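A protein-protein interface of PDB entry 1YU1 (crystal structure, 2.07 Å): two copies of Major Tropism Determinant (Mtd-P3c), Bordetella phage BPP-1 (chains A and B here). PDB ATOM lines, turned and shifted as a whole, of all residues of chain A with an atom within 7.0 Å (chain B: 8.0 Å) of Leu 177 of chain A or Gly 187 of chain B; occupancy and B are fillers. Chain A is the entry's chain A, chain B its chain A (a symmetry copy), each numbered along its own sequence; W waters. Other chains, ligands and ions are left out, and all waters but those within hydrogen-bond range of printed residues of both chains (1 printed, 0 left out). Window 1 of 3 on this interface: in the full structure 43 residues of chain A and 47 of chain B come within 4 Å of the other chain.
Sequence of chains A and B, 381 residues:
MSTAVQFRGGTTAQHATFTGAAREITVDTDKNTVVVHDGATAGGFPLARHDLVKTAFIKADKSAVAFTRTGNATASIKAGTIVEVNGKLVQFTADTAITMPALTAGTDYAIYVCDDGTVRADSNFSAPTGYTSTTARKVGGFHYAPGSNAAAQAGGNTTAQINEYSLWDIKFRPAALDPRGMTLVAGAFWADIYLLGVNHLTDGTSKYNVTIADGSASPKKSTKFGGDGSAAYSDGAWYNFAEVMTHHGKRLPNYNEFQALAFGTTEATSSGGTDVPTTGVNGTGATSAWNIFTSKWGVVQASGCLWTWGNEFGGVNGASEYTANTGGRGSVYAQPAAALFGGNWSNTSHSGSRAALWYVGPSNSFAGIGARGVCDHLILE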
ATOM      1  N   ARG A 173     -14.511 -31.671 -21.231  1.00  0.00           N
ATOM      2  CA  ARG A 173     -13.257 -32.238 -20.769  1.00  0.00           C
ATOM      3  C   ARG A 173     -13.055 -32.092 -19.261  1.00  0.00           C
ATOM      4  O   ARG A 173     -13.754 -31.313 -18.600  1.00  0.00           O
ATOM      5  CB  ARG A 173     -12.090 -31.562 -21.505  1.00  0.00           C
ATOM      6  CG  ARG A 173     -12.097 -30.030 -21.462  1.00  0.00           C
ATOM      7  CD  ARG A 173     -10.742 -29.408 -21.813  1.00  0.00           C
ATOM      8  NE  ARG A 173      -9.763 -29.760 -20.789  1.00  0.00           N
ATOM      9  CZ  ARG A 173      -8.451 -29.936 -20.983  1.00  0.00           C
ATOM     10  NH1 ARG A 173      -7.887 -29.745 -22.172  1.00  0.00           N
ATOM     11  NH2 ARG A 173      -7.692 -30.285 -19.942  1.00  0.00           N
ATOM     12  N   PRO A 174     -12.093 -32.839 -18.721  1.00  0.00           N
ATOM     13  CA  PRO A 174     -11.663 -32.613 -17.343  1.00  0.00           C
ATOM     14  C   PRO A 174     -11.057 -31.228 -17.230  1.00  0.00           C
ATOM     15  O   PRO A 174     -10.448 -30.747 -18.191  1.00  0.00           O
ATOM     16  CB  PRO A 174     -10.602 -33.697 -17.110  1.00  0.00           C
ATOM     17  CG  PRO A 174     -10.184 -34.141 -18.455  1.00  0.00           C
ATOM     18  CD  PRO A 174     -11.340 -33.938 -19.356  1.00  0.00           C
ATOM     19  N   ALA A 175     -11.229 -30.600 -16.071  1.00  0.00           N
ATOM     20  CA  ALA A 175     -10.633 -29.297 -15.812  1.00  0.00           C
ATOM     21  C   ALA A 175      -9.142 -29.429 -15.494  1.00  0.00           C
ATOM     22  O   ALA A 175      -8.460 -28.424 -15.325  1.00  0.00           O
ATOM     23  CB  ALA A 175     -11.357 -28.604 -14.666  1.00  0.00           C
ATOM     24  N   ALA A 176      -8.634 -30.658 -15.406  1.00  0.00           N
ATOM     25  CA  ALA A 176      -7.223 -30.870 -15.096  1.00  0.00           C
ATOM     26  C   ALA A 176      -6.341 -30.292 -16.189  1.00  0.00           C
ATOM     27  O   ALA A 176      -6.768 -30.119 -17.325  1.00  0.00           O
ATOM     28  CB  ALA A 176      -6.934 -32.340 -14.918  1.00  0.00           C
ATOM     29  N   LEU A 177      -5.091 -30.032 -15.838  1.00  0.00           N
ATOM     30  CA  LEU A 177      -4.136 -29.436 -16.764  1.00  0.00           C
ATOM     31  C   LEU A 177      -3.864 -30.360 -17.959  1.00  0.00           C
ATOM     32  O   LEU A 177      -3.570 -29.893 -19.059  1.00  0.00           O
ATOM     33  CB  LEU A 177      -2.832 -29.087 -16.021  1.00  0.00           C
ATOM     34  CG  LEU A 177      -2.982 -28.398 -14.648  1.00  0.00           C
ATOM     35  CD1 LEU A 177      -1.630 -28.150 -13.974  1.00  0.00           C
ATOM     36  CD2 LEU A 177      -3.762 -27.100 -14.774  1.00  0.00           C
ATOM     37  N   ASP A 178      -3.991 -31.668 -17.730  1.00  0.00           N
ATOM     38  CA  ASP A 178      -3.783 -32.696 -18.748  1.00  0.00           C
ATOM     39  C   ASP A 178      -4.973 -33.666 -18.694  1.00  0.00           C
ATOM     40  O   ASP A 178      -5.227 -34.273 -17.645  1.00  0.00           O
ATOM     41  CB  ASP A 178      -2.472 -33.427 -18.442  1.00  0.00           C
ATOM     42  CG  ASP A 178      -2.099 -34.467 -19.488  1.00  0.00           C
ATOM     43  OD1 ASP A 178      -0.967 -34.996 -19.388  1.00  0.00           O
ATOM     44  OD2 ASP A 178      -2.842 -34.836 -20.420  1.00  0.00           O
ATOM     45  N   PRO A 179      -5.720 -33.796 -19.790  1.00  0.00           N
ATOM     46  CA  PRO A 179      -6.907 -34.663 -19.807  1.00  0.00           C
ATOM     47  C   PRO A 179      -6.633 -36.160 -19.973  1.00  0.00           C
ATOM     48  O   PRO A 179      -7.544 -36.951 -19.741  1.00  0.00           O
ATOM     49  CB  PRO A 179      -7.682 -34.152 -21.020  1.00  0.00           C
ATOM     50  CG  PRO A 179      -6.618 -33.674 -21.958  1.00  0.00           C
ATOM     51  CD  PRO A 179      -5.526 -33.112 -21.084  1.00  0.00           C
ATOM     52  N   ARG A 180      -5.420 -36.541 -20.367  1.00  0.00           N
ATOM     53  CA  ARG A 180      -5.115 -37.936 -20.694  1.00  0.00           C
ATOM     54  C   ARG A 180      -5.319 -38.923 -19.532  1.00  0.00           C
ATOM     55  O   ARG A 180      -4.983 -38.636 -18.386  1.00  0.00           O
ATOM     56  CB  ARG A 180      -3.678 -38.061 -21.190  1.00  0.00           C
ATOM     57  CG  ARG A 180      -3.440 -37.496 -22.574  1.00  0.00           C
ATOM     58  CD  ARG A 180      -1.988 -37.572 -23.003  1.00  0.00           C
ATOM     59  NE  ARG A 180      -1.165 -36.572 -22.322  1.00  0.00           N
ATOM     60  CZ  ARG A 180       0.066 -36.228 -22.698  1.00  0.00           C
ATOM     61  NH1 ARG A 180       0.645 -36.809 -23.740  1.00  0.00           N
ATOM     62  NH2 ARG A 180       0.730 -35.298 -22.018  1.00  0.00           N
ATOM     63  N   LYS A 224       6.896 -28.807  -8.457  1.00  0.00           N
ATOM     64  CA  LYS A 224       6.266 -27.550  -8.036  1.00  0.00           C
ATOM     65  C   LYS A 224       6.384 -27.303  -6.522  1.00  0.00           C
ATOM     66  O   LYS A 224       6.049 -26.215  -6.041  1.00  0.00           O
ATOM     67  CB  LYS A 224       4.788 -27.536  -8.437  1.00  0.00           C
ATOM     68  CG  LYS A 224       4.545 -27.494  -9.929  1.00  0.00           C
ATOM     69  CD  LYS A 224       3.077 -27.233 -10.237  1.00  0.00           C
ATOM     70  CE  LYS A 224       2.769 -27.447 -11.719  1.00  0.00           C
ATOM     71  NZ  LYS A 224       1.298 -27.487 -11.994  1.00  0.00           N
ATOM     72  N   THR A 246      -2.410 -32.049  -6.591  1.00  0.00           N
ATOM     73  CA  THR A 246      -2.418 -30.601  -6.791  1.00  0.00           C
ATOM     74  C   THR A 246      -1.460 -30.173  -7.909  1.00  0.00           C
ATOM     75  O   THR A 246      -1.795 -29.304  -8.707  1.00  0.00           O
ATOM     76  CB  THR A 246      -2.056 -29.882  -5.471  1.00  0.00           C
ATOM     77  OG1 THR A 246      -3.067 -30.139  -4.482  1.00  0.00           O
ATOM     78  CG2 THR A 246      -2.077 -28.360  -5.639  1.00  0.00           C
ATOM     79  N   HIS A 247      -0.279 -30.792  -7.949  1.00  0.00           N
ATOM     80  CA  HIS A 247       0.707 -30.596  -9.015  1.00  0.00           C
ATOM     81  C   HIS A 247       0.056 -30.695 -10.394  1.00  0.00           C
ATOM     82  O   HIS A 247       0.343 -29.892 -11.279  1.00  0.00           O
ATOM     83  CB  HIS A 247       1.825 -31.652  -8.897  1.00  0.00           C
ATOM     84  CG  HIS A 247       2.884 -31.554  -9.954  1.00  0.00           C
ATOM     85  ND1 HIS A 247       2.599 -31.294 -11.277  1.00  0.00           N
ATOM     86  CD2 HIS A 247       4.227 -31.699  -9.887  1.00  0.00           C
ATOM     87  CE1 HIS A 247       3.721 -31.267 -11.973  1.00  0.00           C
ATOM     88  NE2 HIS A 247       4.724 -31.515 -11.153  1.00  0.00           N
ATOM     89  N   HIS A 248      -0.808 -31.693 -10.556  1.00  0.00           N
ATOM     90  CA  HIS A 248      -1.439 -31.999 -11.836  1.00  0.00           C
ATOM     91  C   HIS A 248      -2.836 -31.385 -11.992  1.00  0.00           C
ATOM     92  O   HIS A 248      -3.539 -31.682 -12.954  1.00  0.00           O
ATOM     93  CB  HIS A 248      -1.509 -33.522 -12.012  1.00  0.00           C
ATOM     94  CG  HIS A 248      -0.168 -34.181 -12.158  1.00  0.00           C
ATOM     95  ND1 HIS A 248       0.466 -34.825 -11.116  1.00  0.00           N
ATOM     96  CD2 HIS A 248       0.651 -34.306 -13.228  1.00  0.00           C
ATOM     97  CE1 HIS A 248       1.619 -35.312 -11.539  1.00  0.00           C
ATOM     98  NE2 HIS A 248       1.754 -35.012 -12.818  1.00  0.00           N
ATOM     99  N   GLY A 249      -3.246 -30.538 -11.048  1.00  0.00           N
ATOM    100  CA  GLY A 249      -4.530 -29.854 -11.134  1.00  0.00           C
ATOM    101  C   GLY A 249      -5.708 -30.764 -10.837  1.00  0.00           C
ATOM    102  O   GLY A 249      -6.797 -30.564 -11.356  1.00  0.00           O
ATOM    103  N   LYS A 250      -5.473 -31.762  -9.996  1.00  0.00           N
ATOM    104  CA  LYS A 250      -6.472 -32.753  -9.623  1.00  0.00           C
ATOM    105  C   LYS A 250      -6.594 -32.761  -8.107  1.00  0.00           C
ATOM    106  O   LYS A 250      -5.890 -32.011  -7.402  1.00  0.00           O
ATOM    107  CB  LYS A 250      -6.043 -34.143 -10.125  1.00  0.00           C
ATOM    108  CG  LYS A 250      -5.733 -34.192 -11.618  1.00  0.00           C
ATOM    109  CD  LYS A 250      -5.438 -35.599 -12.119  1.00  0.00           C
ATOM    110  CE  LYS A 250      -5.355 -35.623 -13.631  1.00  0.00           C
ATOM    111  NZ  LYS A 250      -4.891 -36.934 -14.177  1.00  0.00           N
ATOM    112  N   CYS A 375     -11.035 -34.546 -11.086  1.00  0.00           N
ATOM    113  CA  CYS A 375     -11.269 -33.065 -11.117  1.00  0.00           C
ATOM    114  C   CYS A 375     -12.663 -32.857 -11.737  1.00  0.00           C
ATOM    115  O   CYS A 375     -13.367 -33.820 -12.059  1.00  0.00           O
ATOM    116  CB  CYS A 375     -10.144 -32.191 -11.833  1.00  0.00           C
ATOM    117  SG  CYS A 375      -9.487 -30.594 -10.973  1.00  0.00           S
ATOM    118  N   SER B  63      -3.668 -22.319 -22.194  1.00  0.00           N
ATOM    119  CA  SER B  63      -3.329 -22.942 -20.906  1.00  0.00           C
ATOM    120  C   SER B  63      -2.432 -22.079 -20.003  1.00  0.00           C
ATOM    121  O   SER B  63      -2.138 -22.466 -18.872  1.00  0.00           O
ATOM    122  CB  SER B  63      -2.653 -24.299 -21.140  1.00  0.00           C
ATOM    123  OG  SER B  63      -1.296 -24.143 -21.534  1.00  0.00           O
ATOM    124  N   TYR B 165       2.717 -14.834 -10.322  1.00  0.00           N
ATOM    125  CA  TYR B 165       1.609 -15.779 -10.161  1.00  0.00           C
ATOM    126  C   TYR B 165       0.268 -15.088  -9.963  1.00  0.00           C
ATOM    127  O   TYR B 165      -0.775 -15.731 -10.009  1.00  0.00           O
ATOM    128  CB  TYR B 165       1.898 -16.720  -8.983  1.00  0.00           C
ATOM    129  CG  TYR B 165       3.078 -17.638  -9.219  1.00  0.00           C
ATOM    130  CD1 TYR B 165       3.088 -18.536 -10.288  1.00  0.00           C
ATOM    131  CD2 TYR B 165       4.187 -17.615  -8.372  1.00  0.00           C
ATOM    132  CE1 TYR B 165       4.177 -19.390 -10.508  1.00  0.00           C
ATOM    133  CE2 TYR B 165       5.271 -18.465  -8.579  1.00  0.00           C
ATOM    134  CZ  TYR B 165       5.259 -19.349  -9.648  1.00  0.00           C
ATOM    135  OH  TYR B 165       6.332 -20.188  -9.855  1.00  0.00           O
ATOM    136  N   PHE B 172      -8.290 -16.669 -17.938  1.00  0.00           N
ATOM    137  CA  PHE B 172      -7.285 -17.334 -17.113  1.00  0.00           C
ATOM    138  C   PHE B 172      -7.260 -16.591 -15.779  1.00  0.00           C
ATOM    139  O   PHE B 172      -6.494 -15.648 -15.596  1.00  0.00           O
ATOM    140  CB  PHE B 172      -5.914 -17.290 -17.792  1.00  0.00           C
ATOM    141  CG  PHE B 172      -4.867 -18.121 -17.105  1.00  0.00           C
ATOM    142  CD1 PHE B 172      -4.664 -19.439 -17.472  1.00  0.00           C
ATOM    143  CD2 PHE B 172      -4.072 -17.578 -16.100  1.00  0.00           C
ATOM    144  CE1 PHE B 172      -3.692 -20.208 -16.846  1.00  0.00           C
ATOM    145  CE2 PHE B 172      -3.102 -18.336 -15.471  1.00  0.00           C
ATOM    146  CZ  PHE B 172      -2.913 -19.658 -15.845  1.00  0.00           C
ATOM    147  N   THR B 183      -3.553 -14.903  -6.026  1.00  0.00           N
ATOM    148  CA  THR B 183      -2.415 -15.514  -6.714  1.00  0.00           C
ATOM    149  C   THR B 183      -2.652 -16.991  -7.055  1.00  0.00           C
ATOM    150  O   THR B 183      -3.327 -17.707  -6.321  1.00  0.00           O
ATOM    151  CB  THR B 183      -1.127 -15.345  -5.883  1.00  0.00           C
ATOM    152  OG1 THR B 183      -0.020 -15.934  -6.581  1.00  0.00           O
ATOM    153  CG2 THR B 183      -1.199 -16.110  -4.549  1.00  0.00           C
ATOM    154  N   LEU B 184      -2.075 -17.437  -8.172  1.00  0.00           N
ATOM    155  CA  LEU B 184      -2.290 -18.786  -8.684  1.00  0.00           C
ATOM    156  C   LEU B 184      -1.304 -19.763  -8.047  1.00  0.00           C
ATOM    157  O   LEU B 184      -0.091 -19.662  -8.246  1.00  0.00           O
ATOM    158  CB  LEU B 184      -2.176 -18.815 -10.215  1.00  0.00           C
ATOM    159  CG  LEU B 184      -2.384 -20.172 -10.901  1.00  0.00           C
ATOM    160  CD1 LEU B 184      -3.613 -20.896 -10.360  1.00  0.00           C
ATOM    161  CD2 LEU B 184      -2.466 -20.026 -12.408  1.00  0.00           C
ATOM    162  N   VAL B 185      -1.842 -20.697  -7.262  1.00  0.00           N
ATOM    163  CA  VAL B 185      -1.053 -21.678  -6.533  1.00  0.00           C
ATOM    164  C   VAL B 185      -0.861 -22.945  -7.366  1.00  0.00           C
ATOM    165  O   VAL B 185      -1.803 -23.708  -7.552  1.00  0.00           O
ATOM    166  CB  VAL B 185      -1.747 -22.057  -5.209  1.00  0.00           C
ATOM    167  CG1 VAL B 185      -0.964 -23.145  -4.476  1.00  0.00           C
ATOM    168  CG2 VAL B 185      -1.935 -20.818  -4.323  1.00  0.00           C
ATOM    169  N   ALA B 186       0.363 -23.152  -7.856  1.00  0.00           N
ATOM    170  CA  ALA B 186       0.759 -24.378  -8.553  1.00  0.00           C
ATOM    171  C   ALA B 186      -0.080 -24.670  -9.800  1.00  0.00           C
ATOM    172  O   ALA B 186      -0.179 -25.823 -10.230  1.00  0.00           O
ATOM    173  CB  ALA B 186       0.716 -25.566  -7.593  1.00  0.00           C
ATOM    174  N   GLY B 187      -0.673 -23.620 -10.369  1.00  0.00           N
ATOM    175  CA  GLY B 187      -1.494 -23.718 -11.556  1.00  0.00           C
ATOM    176  C   GLY B 187      -2.873 -24.322 -11.340  1.00  0.00           C
ATOM    177  O   GLY B 187      -3.587 -24.554 -12.315  1.00  0.00           O
ATOM    178  N   ALA B 188      -3.253 -24.528 -10.078  1.00  0.00           N
ATOM    179  CA  ALA B 188      -4.370 -25.396  -9.696  1.00  0.00           C
ATOM    180  C   ALA B 188      -5.598 -24.664  -9.154  1.00  0.00           C
ATOM    181  O   ALA B 188      -6.727 -25.068  -9.424  1.00  0.00           O
ATOM    182  CB  ALA B 188      -3.889 -26.399  -8.645  1.00  0.00           C
ATOM    183  N   PHE B 189      -5.364 -23.649  -8.326  1.00  0.00           N
ATOM    184  CA  PHE B 189      -6.430 -22.836  -7.729  1.00  0.00           C
ATOM    185  C   PHE B 189      -5.852 -21.492  -7.267  1.00  0.00           C
ATOM    186  O   PHE B 189      -4.636 -21.337  -7.189  1.00  0.00           O
ATOM    187  CB  PHE B 189      -7.063 -23.581  -6.546  1.00  0.00           C
ATOM    188  CG  PHE B 189      -6.161 -23.679  -5.353  1.00  0.00           C
ATOM    189  CD1 PHE B 189      -6.210 -22.719  -4.345  1.00  0.00           C
ATOM    190  CD2 PHE B 189      -5.241 -24.718  -5.249  1.00  0.00           C
ATOM    191  CE1 PHE B 189      -5.359 -22.799  -3.247  1.00  0.00           C
ATOM    192  CE2 PHE B 189      -4.384 -24.802  -4.154  1.00  0.00           C
ATOM    193  CZ  PHE B 189      -4.451 -23.841  -3.152  1.00  0.00           C
ATOM    194  N   TRP B 190      -6.714 -20.520  -6.967  1.00  0.00           N
ATOM    195  CA  TRP B 190      -6.267 -19.193  -6.544  1.00  0.00           C
ATOM    196  C   TRP B 190      -6.434 -18.995  -5.039  1.00  0.00           C
ATOM    197  O   TRP B 190      -7.420 -19.440  -4.453  1.00  0.00           O
ATOM    198  CB  TRP B 190      -7.043 -18.095  -7.280  1.00  0.00           C
ATOM    199  CG  TRP B 190      -6.826 -18.101  -8.754  1.00  0.00           C
ATOM    200  CD1 TRP B 190      -7.397 -18.946  -9.660  1.00  0.00           C
ATOM    201  CD2 TRP B 190      -5.982 -17.222  -9.505  1.00  0.00           C
ATOM    202  NE1 TRP B 190      -6.967 -18.642 -10.929  1.00  0.00           N
ATOM    203  CE2 TRP B 190      -6.088 -17.595 -10.862  1.00  0.00           C
ATOM    204  CE3 TRP B 190      -5.138 -16.156  -9.170  1.00  0.00           C
ATOM    205  CZ2 TRP B 190      -5.386 -16.944 -11.877  1.00  0.00           C
ATOM    206  CZ3 TRP B 190      -4.446 -15.511 -10.175  1.00  0.00           C
ATOM    207  CH2 TRP B 190      -4.569 -15.910 -11.513  1.00  0.00           C
ATOM    208  N   TRP B 297       4.186 -18.736  -3.799  1.00  0.00           N
ATOM    209  CA  TRP B 297       3.227 -18.152  -4.716  1.00  0.00           C
ATOM    210  C   TRP B 297       2.852 -16.706  -4.344  1.00  0.00           C
ATOM    211  O   TRP B 297       2.019 -16.075  -5.001  1.00  0.00           O
ATOM    212  CB  TRP B 297       2.052 -19.135  -4.861  1.00  0.00           C
ATOM    213  CG  TRP B 297       2.540 -20.323  -5.710  1.00  0.00           C
ATOM    214  CD1 TRP B 297       2.906 -20.279  -7.028  1.00  0.00           C
ATOM    215  CD2 TRP B 297       2.787 -21.659  -5.285  1.00  0.00           C
ATOM    216  NE1 TRP B 297       3.337 -21.507  -7.461  1.00  0.00           N
ATOM    217  CE2 TRP B 297       3.273 -22.378  -6.410  1.00  0.00           C
ATOM    218  CE3 TRP B 297       2.627 -22.337  -4.083  1.00  0.00           C
ATOM    219  CZ2 TRP B 297       3.599 -23.718  -6.359  1.00  0.00           C
ATOM    220  CZ3 TRP B 297       2.953 -23.657  -4.034  1.00  0.00           C
ATOM    221  CH2 TRP B 297       3.439 -24.344  -5.170  1.00  0.00           C
ATOM    222  N   HIS B 377      -9.576 -22.136 -10.171  1.00  0.00           N
ATOM    223  CA  HIS B 377      -8.948 -21.607 -11.378  1.00  0.00           C
ATOM    224  C   HIS B 377      -9.867 -21.862 -12.567  1.00  0.00           C
ATOM    225  O   HIS B 377     -10.400 -22.960 -12.722  1.00  0.00           O
ATOM    226  CB  HIS B 377      -7.588 -22.272 -11.620  1.00  0.00           C
ATOM    227  CG  HIS B 377      -6.770 -21.604 -12.682  1.00  0.00           C
ATOM    228  ND1 HIS B 377      -6.911 -21.886 -14.020  1.00  0.00           N
ATOM    229  CD2 HIS B 377      -5.803 -20.664 -12.602  1.00  0.00           C
ATOM    230  CE1 HIS B 377      -6.064 -21.143 -14.714  1.00  0.00           C
ATOM    231  NE2 HIS B 377      -5.382 -20.394 -13.877  1.00  0.00           N
ATOM    232  N   LEU B 378     -10.044 -20.839 -13.397  1.00  0.00           N
ATOM    233  CA  LEU B 378     -10.926 -20.902 -14.558  1.00  0.00           C
ATOM    234  C   LEU B 378     -10.131 -20.661 -15.840  1.00  0.00           C
ATOM    235  O   LEU B 378      -9.543 -19.591 -16.011  1.00  0.00           O
ATOM    236  CB  LEU B 378     -12.031 -19.850 -14.432  1.00  0.00           C
ATOM    237  CG  LEU B 378     -13.170 -19.927 -15.458  1.00  0.00           C
ATOM    238  CD1 LEU B 378     -13.794 -21.329 -15.497  1.00  0.00           C
ATOM    239  CD2 LEU B 378     -14.238 -18.875 -15.167  1.00  0.00           C
ATOM    240  N   ILE B 379     -10.101 -21.664 -16.719  1.00  0.00           N
ATOM    241  CA  ILE B 379      -9.498 -21.540 -18.045  1.00  0.00           C
ATOM    242  C   ILE B 379     -10.588 -21.710 -19.088  1.00  0.00           C
ATOM    243  O   ILE B 379     -11.179 -22.787 -19.205  1.00  0.00           O
ATOM    244  CB  ILE B 379      -8.384 -22.591 -18.265  1.00  0.00           C
ATOM    245  CG1 ILE B 379      -7.314 -22.446 -17.187  1.00  0.00           C
ATOM    246  CG2 ILE B 379      -7.736 -22.405 -19.639  1.00  0.00           C
ATOM    247  CD1 ILE B 379      -6.188 -23.469 -17.233  1.00  0.00           C
HETATM  248  O   HOH W   1      -7.392 -27.949  -9.300  1.00  0.00           O
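NZ of Lys 224 of chain A sits at hydrogen-bond distance from O of Ala 186 of chain B.
NZ of Lys 224 of chain A lies within hydrogen-bond range of O of His 247 of chain A (2.7 Å).
OG1 of Thr 183 of chain B sits at hydrogen-bond distance from O of Trp 297 of chain B (2.6 Å).
Among the printed residues, merely in contact across the chains: Lys 224 of chain A with Trp 297 of chain B (3.3 Å), Leu 177 of chain A with Gly 187 of chain B (3.5 Å) and Thr 246 of chain A with Ala 188 of chain B (3.6 Å).
Leu 177 of chain A touches just one residue of chain B: Gly 187 (3.5 Å).
Gly 187 of chain B touches one residue of chain A.
Of the printed residues of chain A, Ala 188 of chain B touches Thr 246 (3.6 Å).
Of the printed residues of chain B, Thr 246 of chain A touches Ala 188.
Of the printed residues of chain A, Ala 186 of chain B touches Lys 224.
Of the printed residues of chain A, Trp 297 of chain B touches Lys 224.
Lys 250 of chain A touches none of the printed residues of chain B.
The nearest residue of chain B that does not touch Leu 177 of chain A is Ala 186 of chain B (4.6 Å).
Printed residues of chain B that touch a printed residue of chain A: Ala 186, Gly 187, Ala 188 and Trp 297.
Hydrophobic or aromatic side chains of chain B that line the printed part of chain A: Ala 186, Ala 188 and Trp 297.
Among the printed residues, 4 pairs touch across the chains.
No position is printed for both chains.
Water W1 bridges O of Ala 188 of chain B (3.0 Å) and O of Gly 249 of chain A (3.4 Å).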
